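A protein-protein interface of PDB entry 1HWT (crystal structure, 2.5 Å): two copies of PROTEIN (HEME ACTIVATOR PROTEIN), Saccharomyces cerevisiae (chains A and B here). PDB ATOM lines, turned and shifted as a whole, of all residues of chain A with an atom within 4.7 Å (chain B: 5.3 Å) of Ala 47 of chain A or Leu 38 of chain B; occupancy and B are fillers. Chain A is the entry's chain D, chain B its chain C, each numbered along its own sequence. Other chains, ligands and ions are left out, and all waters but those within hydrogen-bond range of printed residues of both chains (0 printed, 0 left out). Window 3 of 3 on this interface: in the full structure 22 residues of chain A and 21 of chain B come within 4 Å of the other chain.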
ATOM      1  N   GLU A  43      27.849  -8.694 -17.786  1.00  0.00           N
ATOM      2  CA  GLU A  43      27.207  -7.732 -18.655  1.00  0.00           C
ATOM      3  C   GLU A  43      28.111  -7.419 -19.831  1.00  0.00           C
ATOM      4  O   GLU A  43      29.304  -7.168 -19.667  1.00  0.00           O
ATOM      5  CB  GLU A  43      26.881  -6.451 -17.878  1.00  0.00           C
ATOM      6  CG  GLU A  43      25.389  -6.211 -17.657  1.00  0.00           C
ATOM      7  CD  GLU A  43      24.790  -5.255 -18.683  1.00  0.00           C
ATOM      8  OE1 GLU A  43      24.366  -5.729 -19.767  1.00  0.00           O
ATOM      9  OE2 GLU A  43      24.745  -4.029 -18.410  1.00  0.00           O
ATOM     10  N   GLN A  44      27.527  -7.443 -21.020  1.00  0.00           N
ATOM     11  CA  GLN A  44      28.256  -7.168 -22.247  1.00  0.00           C
ATOM     12  C   GLN A  44      28.062  -5.715 -22.656  1.00  0.00           C
ATOM     13  O   GLN A  44      26.954  -5.199 -22.598  1.00  0.00           O
ATOM     14  CB  GLN A  44      27.760  -8.096 -23.357  1.00  0.00           C
ATOM     15  CG  GLN A  44      28.037  -9.571 -23.113  1.00  0.00           C
ATOM     16  CD  GLN A  44      29.497  -9.917 -23.289  1.00  0.00           C
ATOM     17  OE1 GLN A  44      30.206  -9.270 -24.052  1.00  0.00           O
ATOM     18  NE2 GLN A  44      29.955 -10.940 -22.585  1.00  0.00           N
ATOM     19  N   THR A  45      29.140  -5.062 -23.073  1.00  0.00           N
ATOM     20  CA  THR A  45      29.089  -3.669 -23.472  1.00  0.00           C
ATOM     21  C   THR A  45      28.080  -3.467 -24.595  1.00  0.00           C
ATOM     22  O   THR A  45      27.295  -2.523 -24.569  1.00  0.00           O
ATOM     23  CB  THR A  45      30.486  -3.198 -23.933  1.00  0.00           C
ATOM     24  OG1 THR A  45      31.304  -2.953 -22.782  1.00  0.00           O
ATOM     25  CG2 THR A  45      30.396  -1.922 -24.762  1.00  0.00           C
ATOM     26  N   TRP A  46      28.088  -4.365 -25.574  1.00  0.00           N
ATOM     27  CA  TRP A  46      27.181  -4.255 -26.706  1.00  0.00           C
ATOM     28  C   TRP A  46      25.790  -4.794 -26.434  1.00  0.00           C
ATOM     29  O   TRP A  46      24.948  -4.846 -27.329  1.00  0.00           O
ATOM     30  CB  TRP A  46      27.761  -4.967 -27.926  1.00  0.00           C
ATOM     31  CG  TRP A  46      28.430  -6.275 -27.641  1.00  0.00           C
ATOM     32  CD1 TRP A  46      29.768  -6.525 -27.663  1.00  0.00           C
ATOM     33  CD2 TRP A  46      27.790  -7.540 -27.411  1.00  0.00           C
ATOM     34  NE1 TRP A  46      30.003  -7.860 -27.473  1.00  0.00           N
ATOM     35  CE2 TRP A  46      28.809  -8.508 -27.315  1.00  0.00           C
ATOM     36  CE3 TRP A  46      26.454  -7.946 -27.283  1.00  0.00           C
ATOM     37  CZ2 TRP A  46      28.541  -9.859 -27.098  1.00  0.00           C
ATOM     38  CZ3 TRP A  46      26.186  -9.294 -27.069  1.00  0.00           C
ATOM     39  CH2 TRP A  46      27.226 -10.231 -26.979  1.00  0.00           C
ATOM     40  N   ALA A  47      25.544  -5.205 -25.203  1.00  0.00           N
ATOM     41  CA  ALA A  47      24.235  -5.724 -24.860  1.00  0.00           C
ATOM     42  C   ALA A  47      23.520  -4.740 -23.951  1.00  0.00           C
ATOM     43  O   ALA A  47      22.309  -4.752 -23.868  1.00  0.00           O
ATOM     44  CB  ALA A  47      24.382  -7.070 -24.171  1.00  0.00           C
ATOM     45  N   GLU A  48      24.278  -3.880 -23.283  1.00  0.00           N
ATOM     46  CA  GLU A  48      23.718  -2.907 -22.349  1.00  0.00           C
ATOM     47  C   GLU A  48      22.417  -2.270 -22.803  1.00  0.00           C
ATOM     48  O   GLU A  48      21.438  -2.260 -22.059  1.00  0.00           O
ATOM     49  CB  GLU A  48      24.737  -1.794 -22.060  1.00  0.00           C
ATOM     50  CG  GLU A  48      24.971  -1.503 -20.566  1.00  0.00           C
ATOM     51  CD  GLU A  48      23.717  -1.003 -19.832  1.00  0.00           C
ATOM     52  OE1 GLU A  48      22.695  -1.750 -19.790  1.00  0.00           O
ATOM     53  OE2 GLU A  48      23.750   0.140 -19.290  1.00  0.00           O
ATOM     54  N   GLU A  49      22.404  -1.739 -24.022  1.00  0.00           N
ATOM     55  CA  GLU A  49      21.230  -1.071 -24.561  1.00  0.00           C
ATOM     56  C   GLU A  49      20.050  -2.020 -24.733  1.00  0.00           C
ATOM     57  O   GLU A  49      18.933  -1.700 -24.346  1.00  0.00           O
ATOM     58  CB  GLU A  49      21.582  -0.414 -25.896  1.00  0.00           C
ATOM     59  CG  GLU A  49      22.747   0.578 -25.815  1.00  0.00           C
ATOM     60  CD  GLU A  49      24.112  -0.016 -26.226  1.00  0.00           C
ATOM     61  OE1 GLU A  49      24.537  -1.030 -25.619  1.00  0.00           O
ATOM     62  OE2 GLU A  49      24.768   0.544 -27.146  1.00  0.00           O
ATOM     63  N   ALA A  50      20.300  -3.187 -25.314  1.00  0.00           N
ATOM     64  CA  ALA A  50      19.249  -4.175 -25.522  1.00  0.00           C
ATOM     65  C   ALA A  50      18.708  -4.683 -24.182  1.00  0.00           C
ATOM     66  O   ALA A  50      17.547  -5.094 -24.083  1.00  0.00           O
ATOM     67  CB  ALA A  50      19.773  -5.329 -26.346  1.00  0.00           C
ATOM     68  N   GLU A  51      19.562  -4.653 -23.162  1.00  0.00           N
ATOM     69  CA  GLU A  51      19.190  -5.089 -21.818  1.00  0.00           C
ATOM     70  C   GLU A  51      18.309  -4.023 -21.182  1.00  0.00           C
ATOM     71  O   GLU A  51      17.244  -4.311 -20.645  1.00  0.00           O
ATOM     72  CB  GLU A  51      20.445  -5.275 -20.956  1.00  0.00           C
ATOM     73  CG  GLU A  51      20.433  -6.515 -20.082  1.00  0.00           C
ATOM     74  CD  GLU A  51      21.321  -7.603 -20.645  1.00  0.00           C
ATOM     75  OE1 GLU A  51      22.564  -7.450 -20.522  1.00  0.00           O
ATOM     76  OE2 GLU A  51      20.784  -8.600 -21.216  1.00  0.00           O
ATOM     77  N   LEU A  54      14.832  -4.382 -22.688  1.00  0.00           N
ATOM     78  CA  LEU A  54      14.064  -5.530 -22.225  1.00  0.00           C
ATOM     79  C   LEU A  54      13.539  -5.319 -20.814  1.00  0.00           C
ATOM     80  O   LEU A  54      12.365  -5.556 -20.550  1.00  0.00           O
ATOM     81  CB  LEU A  54      14.932  -6.777 -22.247  1.00  0.00           C
ATOM     82  CG  LEU A  54      14.313  -8.083 -22.737  1.00  0.00           C
ATOM     83  CD1 LEU A  54      13.882  -7.953 -24.195  1.00  0.00           C
ATOM     84  CD2 LEU A  54      15.341  -9.191 -22.563  1.00  0.00           C
ATOM     85  N   THR B  11      20.266  -5.271 -34.006  1.00  0.00           N
ATOM     86  CA  THR B  11      21.054  -4.296 -33.278  1.00  0.00           C
ATOM     87  C   THR B  11      22.327  -4.852 -32.650  1.00  0.00           C
ATOM     88  O   THR B  11      23.353  -4.185 -32.649  1.00  0.00           O
ATOM     89  CB  THR B  11      20.207  -3.610 -32.174  1.00  0.00           C
ATOM     90  OG1 THR B  11      19.426  -4.587 -31.473  1.00  0.00           O
ATOM     91  CG2 THR B  11      19.288  -2.580 -32.783  1.00  0.00           C
ATOM     92  N   ILE B  12      22.276  -6.069 -32.118  1.00  0.00           N
ATOM     93  CA  ILE B  12      23.455  -6.637 -31.479  1.00  0.00           C
ATOM     94  C   ILE B  12      24.595  -6.879 -32.456  1.00  0.00           C
ATOM     95  O   ILE B  12      25.737  -6.528 -32.166  1.00  0.00           O
ATOM     96  CB  ILE B  12      23.134  -7.961 -30.762  1.00  0.00           C
ATOM     97  CG1 ILE B  12      22.134  -7.712 -29.629  1.00  0.00           C
ATOM     98  CG2 ILE B  12      24.412  -8.591 -30.230  1.00  0.00           C
ATOM     99  CD1 ILE B  12      22.598  -6.715 -28.610  1.00  0.00           C
ATOM    100  N   CYS B  30      23.371 -14.262 -32.469  1.00  0.00           N
ATOM    101  CA  CYS B  30      22.931 -14.012 -31.115  1.00  0.00           C
ATOM    102  C   CYS B  30      22.632 -15.359 -30.494  1.00  0.00           C
ATOM    103  O   CYS B  30      22.985 -15.620 -29.351  1.00  0.00           O
ATOM    104  CB  CYS B  30      21.648 -13.178 -31.108  1.00  0.00           C
ATOM    105  SG  CYS B  30      21.846 -11.401 -31.409  1.00  0.00           S
ATOM    106  N   VAL B  35      22.638 -14.935 -26.601  1.00  0.00           N
ATOM    107  CA  VAL B  35      21.910 -13.703 -26.335  1.00  0.00           C
ATOM    108  C   VAL B  35      20.667 -13.504 -27.194  1.00  0.00           C
ATOM    109  O   VAL B  35      20.249 -12.373 -27.438  1.00  0.00           O
ATOM    110  CB  VAL B  35      22.851 -12.475 -26.494  1.00  0.00           C
ATOM    111  CG1 VAL B  35      23.885 -12.485 -25.385  1.00  0.00           C
ATOM    112  CG2 VAL B  35      23.544 -12.501 -27.836  1.00  0.00           C
ATOM    113  N   ALA B  36      20.071 -14.602 -27.642  1.00  0.00           N
ATOM    114  CA  ALA B  36      18.875 -14.553 -28.482  1.00  0.00           C
ATOM    115  C   ALA B  36      17.765 -13.721 -27.882  1.00  0.00           C
ATOM    116  O   ALA B  36      17.003 -13.088 -28.597  1.00  0.00           O
ATOM    117  CB  ALA B  36      18.371 -15.950 -28.746  1.00  0.00           C
ATOM    118  N   HIS B  37      17.668 -13.717 -26.564  1.00  0.00           N
ATOM    119  CA  HIS B  37      16.633 -12.948 -25.898  1.00  0.00           C
ATOM    120  C   HIS B  37      16.875 -11.457 -26.053  1.00  0.00           C
ATOM    121  O   HIS B  37      16.025 -10.646 -25.686  1.00  0.00           O
ATOM    122  CB  HIS B  37      16.593 -13.303 -24.417  1.00  0.00           C
ATOM    123  CG  HIS B  37      17.804 -12.861 -23.663  1.00  0.00           C
ATOM    124  ND1 HIS B  37      19.054 -13.392 -23.890  1.00  0.00           N
ATOM    125  CD2 HIS B  37      17.961 -11.933 -22.685  1.00  0.00           C
ATOM    126  CE1 HIS B  37      19.932 -12.814 -23.085  1.00  0.00           C
ATOM    127  NE2 HIS B  37      19.293 -11.925 -22.346  1.00  0.00           N
ATOM    128  N   LEU B  38      18.041 -11.089 -26.570  1.00  0.00           N
ATOM    129  CA  LEU B  38      18.362  -9.677 -26.751  1.00  0.00           C
ATOM    130  C   LEU B  38      18.407  -9.334 -28.225  1.00  0.00           C
ATOM    131  O   LEU B  38      18.677  -8.206 -28.603  1.00  0.00           O
ATOM    132  CB  LEU B  38      19.716  -9.344 -26.116  1.00  0.00           C
ATOM    133  CG  LEU B  38      19.924  -9.588 -24.622  1.00  0.00           C
ATOM    134  CD1 LEU B  38      21.276  -9.035 -24.230  1.00  0.00           C
ATOM    135  CD2 LEU B  38      18.822  -8.940 -23.808  1.00  0.00           C
ATOM    136  N   CYS B  39      18.124 -10.321 -29.060  1.00  0.00           N
ATOM    137  CA  CYS B  39      18.163 -10.112 -30.500  1.00  0.00           C
ATOM    138  C   CYS B  39      16.865  -9.574 -31.021  1.00  0.00           C
ATOM    139  O   CYS B  39      15.832 -10.224 -30.902  1.00  0.00           O
ATOM    140  CB  CYS B  39      18.454 -11.408 -31.241  1.00  0.00           C
ATOM    141  SG  CYS B  39      18.478 -11.152 -33.034  1.00  0.00           S
ATOM    142  N   HIS B  40      16.918  -8.386 -31.607  1.00  0.00           N
ATOM    143  CA  HIS B  40      15.727  -7.780 -32.165  1.00  0.00           C
ATOM    144  C   HIS B  40      16.107  -6.922 -33.349  1.00  0.00           C
ATOM    145  O   HIS B  40      17.244  -6.450 -33.445  1.00  0.00           O
ATOM    146  CB  HIS B  40      14.986  -6.959 -31.105  1.00  0.00           C
ATOM    147  CG  HIS B  40      15.739  -5.763 -30.618  1.00  0.00           C
ATOM    148  ND1 HIS B  40      15.595  -4.512 -31.179  1.00  0.00           N
ATOM    149  CD2 HIS B  40      16.614  -5.619 -29.595  1.00  0.00           C
ATOM    150  CE1 HIS B  40      16.347  -3.648 -30.521  1.00  0.00           C
ATOM    151  NE2 HIS B  40      16.977  -4.293 -29.554  1.00  0.00           N
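The side-chain carboxylate (OE1) of Glu 51 of chain A sits close to the side-chain carboxylate (OE1) of Glu 43 of chain A (2.6 Å).
Trp 46 of chain A touches Ile 12 of chain B.
Ala 47 of chain A touches Leu 38 of chain B (CB to CD1, 3.7 Å).
Ala 50 of chain A touches Ile 12 of chain B.
Ala 50 of chain A touches Leu 38 of chain B.
Glu 51 of chain A touches His 37 of chain B.
Leu 38 of chain B touches Glu 51 of chain A.
His 37 of chain B touches Leu 54 of chain A.
CD2 of Leu 38 of chain B touches CD2 of Leu 54 of chain A, 3.7 Å away.
Ala 47 of chain A touches just one residue of chain B: Leu 38 (3.7 Å).
Printed residues of chain A within 4 Å of Ile 12 of chain B: Trp 46 and Ala 50.
Printed residues of chain A within 4 Å of His 37 of chain B: Glu 51 and Leu 54.
The nearest printed residue of chain A that does not touch Leu 38 of chain B is Trp 46 of chain A (5.7 Å).
Hydrophobic or aromatic side chains of chain B that line the printed part of chain A: Ile 12, His 37 and Leu 38.
Among the printed residues, no Asp or Glu carboxylate lies within 4 Å of a Lys or Arg side-chain nitrogen of the other chain.
No position is printed for both chains.
Of the 8 pairs that touch across the chains among the printed residues, none has its exchanged pair printed and touching as well.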
